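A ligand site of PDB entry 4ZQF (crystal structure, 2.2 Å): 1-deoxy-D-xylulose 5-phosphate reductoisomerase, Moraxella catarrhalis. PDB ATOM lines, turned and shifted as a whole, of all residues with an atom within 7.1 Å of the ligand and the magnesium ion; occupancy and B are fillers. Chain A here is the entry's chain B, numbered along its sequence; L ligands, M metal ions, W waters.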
ATOM      1  N   LYS A 146     -22.574   3.707   4.388  1.00  0.00           N
ATOM      2  CA  LYS A 146     -21.727   2.573   4.622  1.00  0.00           C
ATOM      3  C   LYS A 146     -22.492   1.250   4.543  1.00  0.00           C
ATOM      4  O   LYS A 146     -21.946   0.220   4.100  1.00  0.00           O
ATOM      5  CB  LYS A 146     -20.987   2.755   5.963  1.00  0.00           C
ATOM      6  CG  LYS A 146     -20.216   4.074   6.019  1.00  0.00           C
ATOM      7  CD  LYS A 146     -18.916   4.018   6.851  1.00  0.00           C
ATOM      8  CE  LYS A 146     -18.010   5.252   6.645  1.00  0.00           C
ATOM      9  NZ  LYS A 146     -17.623   5.483   5.206  1.00  0.00           N
ATOM     10  N   ILE A 170     -18.334   8.086  -2.771  1.00  0.00           N
ATOM     11  CA  ILE A 170     -18.350   9.520  -2.447  1.00  0.00           C
ATOM     12  C   ILE A 170     -17.656   9.776  -1.139  1.00  0.00           C
ATOM     13  O   ILE A 170     -17.171  10.872  -0.916  1.00  0.00           O
ATOM     14  CB  ILE A 170     -19.794  10.024  -2.320  1.00  0.00           C
ATOM     15  CG1 ILE A 170     -20.303  10.485  -3.674  1.00  0.00           C
ATOM     16  CG2 ILE A 170     -19.977  11.105  -1.251  1.00  0.00           C
ATOM     17  CD1 ILE A 170     -21.821  10.578  -3.678  1.00  0.00           C
ATOM     18  N   ASP A 171     -17.689   8.807  -0.228  1.00  0.00           N
ATOM     19  CA  ASP A 171     -16.969   8.987   1.007  1.00  0.00           C
ATOM     20  C   ASP A 171     -15.525   9.283   0.600  1.00  0.00           C
ATOM     21  O   ASP A 171     -14.960   8.691  -0.333  1.00  0.00           O
ATOM     22  CB  ASP A 171     -17.045   7.767   1.920  1.00  0.00           C
ATOM     23  CG  ASP A 171     -16.298   7.956   3.278  1.00  0.00           C
ATOM     24  OD1 ASP A 171     -16.889   8.436   4.277  1.00  0.00           O
ATOM     25  OD2 ASP A 171     -15.127   7.574   3.374  1.00  0.00           O
ATOM     26  N   SER A 172     -14.947  10.171   1.372  1.00  0.00           N
ATOM     27  CA  SER A 172     -13.651  10.783   1.106  1.00  0.00           C
ATOM     28  C   SER A 172     -12.487   9.772   0.890  1.00  0.00           C
ATOM     29  O   SER A 172     -11.741   9.921  -0.051  1.00  0.00           O
ATOM     30  CB  SER A 172     -13.383  11.726   2.279  1.00  0.00           C
ATOM     31  OG  SER A 172     -12.090  12.199   2.218  1.00  0.00           O
ATOM     32  N   GLU A 173     -12.408   8.737   1.725  1.00  0.00           N
ATOM     33  CA  GLU A 173     -11.375   7.723   1.620  1.00  0.00           C
ATOM     34  C   GLU A 173     -11.468   6.867   0.389  1.00  0.00           C
ATOM     35  O   GLU A 173     -10.491   6.735  -0.350  1.00  0.00           O
ATOM     36  CB  GLU A 173     -11.378   6.767   2.835  1.00  0.00           C
ATOM     37  CG  GLU A 173     -10.893   7.393   4.115  1.00  0.00           C
ATOM     38  CD  GLU A 173     -11.958   8.201   4.830  1.00  0.00           C
ATOM     39  OE1 GLU A 173     -11.665   8.843   5.836  1.00  0.00           O
ATOM     40  OE2 GLU A 173     -13.103   8.190   4.409  1.00  0.00           O
ATOM     41  N   HIS A 174     -12.632   6.303   0.171  1.00  0.00           N
ATOM     42  CA  HIS A 174     -12.856   5.454  -0.976  1.00  0.00           C
ATOM     43  C   HIS A 174     -12.720   6.204  -2.301  1.00  0.00           C
ATOM     44  O   HIS A 174     -12.204   5.688  -3.290  1.00  0.00           O
ATOM     45  CB  HIS A 174     -14.213   4.840  -0.845  1.00  0.00           C
ATOM     46  CG  HIS A 174     -14.346   3.968   0.354  1.00  0.00           C
ATOM     47  ND1 HIS A 174     -15.486   3.936   1.132  1.00  0.00           N
ATOM     48  CD2 HIS A 174     -13.461   3.139   0.958  1.00  0.00           C
ATOM     49  CE1 HIS A 174     -15.305   3.109   2.154  1.00  0.00           C
ATOM     50  NE2 HIS A 174     -14.081   2.612   2.067  1.00  0.00           N
ATOM     51  N   THR A 205      -6.450   6.142   5.493  1.00  0.00           N
ATOM     52  CA  THR A 205      -6.045   7.045   6.592  1.00  0.00           C
ATOM     53  C   THR A 205      -7.173   7.306   7.571  1.00  0.00           C
ATOM     54  O   THR A 205      -8.315   7.472   7.205  1.00  0.00           O
ATOM     55  CB  THR A 205      -5.647   8.412   6.055  1.00  0.00           C
ATOM     56  OG1 THR A 205      -6.668   8.828   5.117  1.00  0.00           O
ATOM     57  CG2 THR A 205      -4.290   8.285   5.356  1.00  0.00           C
ATOM     58  N   ALA A 206      -6.797   7.462   8.827  1.00  0.00           N
ATOM     59  CA  ALA A 206      -7.711   7.691   9.870  1.00  0.00           C
ATOM     60  C   ALA A 206      -7.172   8.767  10.813  1.00  0.00           C
ATOM     61  O   ALA A 206      -6.039   8.677  11.221  1.00  0.00           O
ATOM     62  CB  ALA A 206      -7.902   6.361  10.608  1.00  0.00           C
ATOM     63  N   SER A 207      -8.010   9.719  11.220  1.00  0.00           N
ATOM     64  CA  SER A 207      -7.591  10.777  12.126  1.00  0.00           C
ATOM     65  C   SER A 207      -7.269  10.332  13.538  1.00  0.00           C
ATOM     66  O   SER A 207      -6.723  11.115  14.318  1.00  0.00           O
ATOM     67  CB  SER A 207      -8.702  11.788  12.253  1.00  0.00           C
ATOM     68  OG  SER A 207      -9.748  11.248  13.033  1.00  0.00           O
ATOM     69  N   GLY A 208      -7.674   9.117  13.903  1.00  0.00           N
ATOM     70  CA  GLY A 208      -7.466   8.625  15.275  1.00  0.00           C
ATOM     71  C   GLY A 208      -8.487   9.148  16.257  1.00  0.00           C
ATOM     72  O   GLY A 208      -8.375   8.933  17.479  1.00  0.00           O
ATOM     73  N   GLY A 209      -9.487   9.854  15.759  1.00  0.00           N
ATOM     74  CA  GLY A 209     -10.519  10.461  16.621  1.00  0.00           C
ATOM     75  C   GLY A 209     -10.028  11.234  17.817  1.00  0.00           C
ATOM     76  O   GLY A 209      -8.847  11.447  17.972  1.00  0.00           O
ATOM     77  N   SER A 210     -10.943  11.631  18.680  1.00  0.00           N
ATOM     78  CA  SER A 210     -10.654  12.551  19.784  1.00  0.00           C
ATOM     79  C   SER A 210      -9.890  11.979  20.966  1.00  0.00           C
ATOM     80  O   SER A 210      -9.587  12.704  21.912  1.00  0.00           O
ATOM     81  CB  SER A 210     -11.959  13.137  20.293  1.00  0.00           C
ATOM     82  OG  SER A 210     -12.878  12.100  20.599  1.00  0.00           O
ATOM     83  N   MET A 235     -19.464  16.997  11.095  1.00  0.00           N
ATOM     84  CA  MET A 235     -20.479  15.931  11.038  1.00  0.00           C
ATOM     85  C   MET A 235     -20.943  15.384  12.425  1.00  0.00           C
ATOM     86  O   MET A 235     -20.576  15.901  13.508  1.00  0.00           O
ATOM     87  CB  MET A 235     -20.016  14.785  10.112  1.00  0.00           C
ATOM     88  N   ILE A 239     -21.221   9.205  14.042  1.00  0.00           N
ATOM     89  CA  ILE A 239     -20.057   9.132  13.204  1.00  0.00           C
ATOM     90  C   ILE A 239     -18.819   9.675  13.940  1.00  0.00           C
ATOM     91  O   ILE A 239     -17.713   9.185  13.818  1.00  0.00           O
ATOM     92  CB  ILE A 239     -20.361   9.828  11.836  1.00  0.00           C
ATOM     93  CG1 ILE A 239     -19.517   9.228  10.692  1.00  0.00           C
ATOM     94  CG2 ILE A 239     -20.255  11.347  11.952  1.00  0.00           C
ATOM     95  CD1 ILE A 239     -20.191   8.039  10.031  1.00  0.00           C
ATOM     96  N   SER A 240     -19.023  10.674  14.764  1.00  0.00           N
ATOM     97  CA  SER A 240     -17.962  11.223  15.591  1.00  0.00           C
ATOM     98  C   SER A 240     -17.516  10.201  16.687  1.00  0.00           C
ATOM     99  O   SER A 240     -16.313  10.020  16.988  1.00  0.00           O
ATOM    100  CB  SER A 240     -18.431  12.596  16.132  1.00  0.00           C
ATOM    101  OG  SER A 240     -17.708  13.014  17.249  1.00  0.00           O
ATOM    102  N   ASP A 242     -17.913   6.919  16.235  1.00  0.00           N
ATOM    103  CA  ASP A 242     -17.245   5.921  15.422  1.00  0.00           C
ATOM    104  C   ASP A 242     -15.792   6.310  15.100  1.00  0.00           C
ATOM    105  O   ASP A 242     -14.880   5.453  15.005  1.00  0.00           O
ATOM    106  CB  ASP A 242     -18.019   5.677  14.141  1.00  0.00           C
ATOM    107  CG  ASP A 242     -19.295   4.824  14.345  1.00  0.00           C
ATOM    108  OD1 ASP A 242     -19.555   4.339  15.477  1.00  0.00           O
ATOM    109  OD2 ASP A 242     -20.040   4.635  13.376  1.00  0.00           O
ATOM    110  N   SER A 243     -15.575   7.621  14.933  1.00  0.00           N
ATOM    111  CA  SER A 243     -14.229   8.112  14.729  1.00  0.00           C
ATOM    112  C   SER A 243     -13.439   7.904  15.986  1.00  0.00           C
ATOM    113  O   SER A 243     -12.351   7.364  15.913  1.00  0.00           O
ATOM    114  CB  SER A 243     -14.204   9.591  14.342  1.00  0.00           C
ATOM    115  OG  SER A 243     -12.892  10.116  14.540  1.00  0.00           O
ATOM    116  N   ALA A 244     -13.984   8.267  17.138  1.00  0.00           N
ATOM    117  CA  ALA A 244     -13.227   8.057  18.410  1.00  0.00           C
ATOM    118  C   ALA A 244     -12.908   6.617  18.804  1.00  0.00           C
ATOM    119  O   ALA A 244     -11.964   6.390  19.582  1.00  0.00           O
ATOM    120  CB  ALA A 244     -13.934   8.720  19.554  1.00  0.00           C
ATOM    121  N   MET A 246     -12.790   4.099  16.366  1.00  0.00           N
ATOM    122  CA  MET A 246     -12.181   3.643  15.144  1.00  0.00           C
ATOM    123  C   MET A 246     -13.065   2.602  14.474  1.00  0.00           C
ATOM    124  O   MET A 246     -12.637   1.952  13.527  1.00  0.00           O
ATOM    125  CB  MET A 246     -10.788   3.115  15.369  1.00  0.00           C
ATOM    126  CG  MET A 246      -9.948   2.936  14.094  1.00  0.00           C
ATOM    127  SD  MET A 246      -8.816   4.271  13.632  1.00  0.00           S
ATOM    128  CE  MET A 246      -8.127   4.790  15.204  1.00  0.00           C
ATOM    129  N   MET A 247     -14.317   2.488  14.893  1.00  0.00           N
ATOM    130  CA  MET A 247     -15.232   1.650  14.144  1.00  0.00           C
ATOM    131  C   MET A 247     -15.440   2.228  12.773  1.00  0.00           C
ATOM    132  O   MET A 247     -15.539   1.463  11.806  1.00  0.00           O
ATOM    133  CB  MET A 247     -16.570   1.462  14.868  1.00  0.00           C
ATOM    134  CG  MET A 247     -17.458   0.418  14.189  1.00  0.00           C
ATOM    135  SD  MET A 247     -16.808  -1.263  14.087  1.00  0.00           S
ATOM    136  CE  MET A 247     -16.906  -1.642  15.835  1.00  0.00           C
ATOM    137  N   ASN A 248     -15.454   3.551  12.624  1.00  0.00           N
ATOM    138  CA  ASN A 248     -15.599   4.120  11.242  1.00  0.00           C
ATOM    139  C   ASN A 248     -14.605   3.567  10.271  1.00  0.00           C
ATOM    140  O   ASN A 248     -14.962   3.240   9.121  1.00  0.00           O
ATOM    141  CB  ASN A 248     -15.524   5.664  11.246  1.00  0.00           C
ATOM    142  CG  ASN A 248     -15.841   6.266   9.897  1.00  0.00           C
ATOM    143  OD1 ASN A 248     -16.962   6.122   9.369  1.00  0.00           O
ATOM    144  ND2 ASN A 248     -14.851   6.901   9.285  1.00  0.00           N
ATOM    145  N   LYS A 249     -13.343   3.454  10.694  1.00  0.00           N
ATOM    146  CA  LYS A 249     -12.333   2.924   9.800  1.00  0.00           C
ATOM    147  C   LYS A 249     -12.481   1.418   9.547  1.00  0.00           C
ATOM    148  O   LYS A 249     -12.194   0.946   8.437  1.00  0.00           O
ATOM    149  CB  LYS A 249     -10.911   3.251  10.296  1.00  0.00           C
ATOM    150  CG  LYS A 249      -9.907   3.429   9.171  1.00  0.00           C
ATOM    151  CD  LYS A 249     -10.327   4.459   8.130  1.00  0.00           C
ATOM    152  CE  LYS A 249     -10.947   5.711   8.710  1.00  0.00           C
ATOM    153  NZ  LYS A 249     -11.214   6.734   7.645  1.00  0.00           N
ATOM    154  N   GLU A 252     -15.115   1.222   7.053  1.00  0.00           N
ATOM    155  CA  GLU A 252     -14.525   1.572   5.739  1.00  0.00           C
ATOM    156  C   GLU A 252     -13.639   0.458   5.193  1.00  0.00           C
ATOM    157  O   GLU A 252     -13.707   0.127   3.997  1.00  0.00           O
ATOM    158  CB  GLU A 252     -13.786   2.908   5.823  1.00  0.00           C
ATOM    159  CG  GLU A 252     -14.757   4.072   5.764  1.00  0.00           C
ATOM    160  CD  GLU A 252     -14.129   5.401   6.136  1.00  0.00           C
ATOM    161  OE1 GLU A 252     -12.897   5.449   6.301  1.00  0.00           O
ATOM    162  OE2 GLU A 252     -14.874   6.382   6.276  1.00  0.00           O
ATOM    163  N   GLU A 255     -16.077  -2.047   3.657  1.00  0.00           N
ATOM    164  CA  GLU A 255     -16.594  -1.442   2.398  1.00  0.00           C
ATOM    165  C   GLU A 255     -15.567  -1.475   1.267  1.00  0.00           C
ATOM    166  O   GLU A 255     -15.904  -1.781   0.100  1.00  0.00           O
ATOM    167  CB  GLU A 255     -16.913   0.033   2.586  1.00  0.00           C
ATOM    168  CG  GLU A 255     -18.210   0.442   3.219  1.00  0.00           C
ATOM    169  CD  GLU A 255     -18.331   1.962   3.162  1.00  0.00           C
ATOM    170  OE1 GLU A 255     -18.912   2.531   2.160  1.00  0.00           O
ATOM    171  OE2 GLU A 255     -17.746   2.576   4.085  1.00  0.00           O
ATOM    172  N   HIS A 272      -3.441   9.428  10.919  1.00  0.00           N
ATOM    173  CA  HIS A 272      -3.050  10.632  10.265  1.00  0.00           C
ATOM    174  C   HIS A 272      -3.965  11.721  10.787  1.00  0.00           C
ATOM    175  O   HIS A 272      -4.994  11.989  10.233  1.00  0.00           O
ATOM    176  CB  HIS A 272      -3.152  10.409   8.755  1.00  0.00           C
ATOM    177  CG  HIS A 272      -2.985  11.658   7.943  1.00  0.00           C
ATOM    178  ND1 HIS A 272      -2.145  12.665   8.346  1.00  0.00           N
ATOM    179  CD2 HIS A 272      -3.547  12.082   6.785  1.00  0.00           C
ATOM    180  CE1 HIS A 272      -2.212  13.668   7.484  1.00  0.00           C
ATOM    181  NE2 HIS A 272      -3.069  13.347   6.543  1.00  0.00           N
ATOM    182  N   SER A 275      -5.889  14.613   8.754  1.00  0.00           N
ATOM    183  CA  SER A 275      -6.815  14.259   7.658  1.00  0.00           C
ATOM    184  C   SER A 275      -6.637  15.006   6.317  1.00  0.00           C
ATOM    185  O   SER A 275      -7.601  15.163   5.574  1.00  0.00           O
ATOM    186  CB  SER A 275      -8.271  14.351   8.112  1.00  0.00           C
ATOM    187  OG  SER A 275      -8.431  13.708   9.369  1.00  0.00           O
ATOM    188  N   PRO A 295     -11.633  18.918   4.135  1.00  0.00           N
ATOM    189  CA  PRO A 295     -12.808  18.116   4.485  1.00  0.00           C
ATOM    190  C   PRO A 295     -14.059  18.312   3.634  1.00  0.00           C
ATOM    191  O   PRO A 295     -14.992  17.569   3.819  1.00  0.00           O
ATOM    192  CB  PRO A 295     -13.125  18.572   5.911  1.00  0.00           C
ATOM    193  CG  PRO A 295     -11.826  19.103   6.456  1.00  0.00           C
ATOM    194  CD  PRO A 295     -11.195  19.759   5.280  1.00  0.00           C
ATOM    195  N   MET A 297     -16.927  17.953   1.345  1.00  0.00           N
ATOM    196  CA  MET A 297     -17.456  16.850   0.534  1.00  0.00           C
ATOM    197  C   MET A 297     -17.768  17.224  -0.865  1.00  0.00           C
ATOM    198  O   MET A 297     -18.017  16.337  -1.665  1.00  0.00           O
ATOM    199  CB  MET A 297     -18.742  16.262   1.154  1.00  0.00           C
ATOM    200  CG  MET A 297     -18.530  15.523   2.461  1.00  0.00           C
ATOM    201  SD  MET A 297     -17.204  14.315   2.327  1.00  0.00           S
ATOM    202  CE  MET A 297     -17.912  13.166   1.125  1.00  0.00           C
HETATM  203  O1  LIG L   1     -15.413   8.965   7.011  1.00  0.00           O
HETATM  204  N1  LIG L   1     -15.050  10.321   7.122  1.00  0.00           N
HETATM  205  C1  LIG L   1     -14.918  11.082   6.116  1.00  0.00           C
HETATM  206  O2  LIG L   1     -15.058  10.565   5.011  1.00  0.00           O
HETATM  207  C2  LIG L   1     -14.715  10.826   8.441  1.00  0.00           C
HETATM  208  C3  LIG L   1     -13.367  10.136   8.713  1.00  0.00           C
HETATM  209  C4  LIG L   1     -12.928  10.481  10.133  1.00  0.00           C
HETATM  210  P1  LIG L   1     -11.870   9.161  10.678  1.00  0.00           P
HETATM  211  O3  LIG L   1     -10.700   9.125   9.823  1.00  0.00           O
HETATM  212  O4  LIG L   1     -11.549   9.397  12.269  1.00  0.00           O
HETATM  213  O5  LIG L   1     -12.632   7.776  10.427  1.00  0.00           O
HETATM  214 MG    MG M   1     -15.003   8.372   5.372  1.00  0.00          MG
HETATM  215  O   HOH W   1     -10.427   7.537  13.493  1.00  0.00           O
HETATM  216  O   HOH W   2     -12.242   5.700  12.179  1.00  0.00           O
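ND2 of Asn 248 sits at hydrogen-bond distance from O5 of the ligand.
An oxygen (O3) of the ligand sits at hydrogen-bond distance from the backbone NH (N) of Ser 207 (3.1 Å).
O4 of the ligand is in hydrogen-bond range of OG of Ser 207 (2.7 Å).
OG of Ser 243 sits at hydrogen-bond distance from O4 of the ligand, at 2.7 Å.
The side-chain amino group (NZ) of Lys 249 lies within salt-bridge range of an oxygen (O3) of the ligand, 3.3 Å away.
OE1 of Glu 173 is in salt-bridge range of NZ of Lys 249.
The side-chain carboxylate of Glu 252 lies close to the side-chain amide nitrogen of Asn 248.
OE1 of Glu 252 lies within salt-bridge range of NZ of Lys 249 (2.5 Å).
The backbone carbonyl oxygen (O) of Glu 252 lies within hydrogen-bond range of a ring nitrogen (NE2) of His 174.
N of Asn 248 is in hydrogen-bond range of O of Asp 242, 3.1 Å away.
N of Gly 209 lies within hydrogen-bond range of OG of Ser 207 (3.1 Å).
NZ of Lys 249 is in hydrogen-bond range of O of Thr 205.
NZ of Lys 146 lies within salt-bridge range of OE2 of Glu 255 (3.1 Å).
Ser 172 touches the ligand.
O of Thr 205 touches O3 of the ligand, at 3.9 Å.
CA of Ala 206 touches O3 of the ligand, 3.3 Å away.
Of the 28 residues printed, 10 come within 4 Å of the ligand.
Merely in contact with the magnesium ion: Lys 146 (3.9 Å).
The nearest printed residue that does not touch the magnesium ion is Asn 248 (4.2 Å).
The magnesium ion is bound by O1 of the ligand (1.8 Å), OE2 of Glu 173 (2.1 Å), OD2 of Asp 171 (2.2 Å), OD1 of Asp 171 (2.2 Å), OE2 of Glu 252 (2.2 Å) and O2 of the ligand (2.2 Å).
Water W1 lies within hydrogen-bond range of O4 of the ligand (2.5 Å), O of Ser 243 (3.1 Å), N of Gly 208 (3.2 Å), N of Gly 209 (3.4 Å) and SD of Met 246 (3.6 Å).
Water W2 lies within hydrogen-bond range of an oxygen (O5) of the ligand and the backbone NH (N) of Lys 249.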
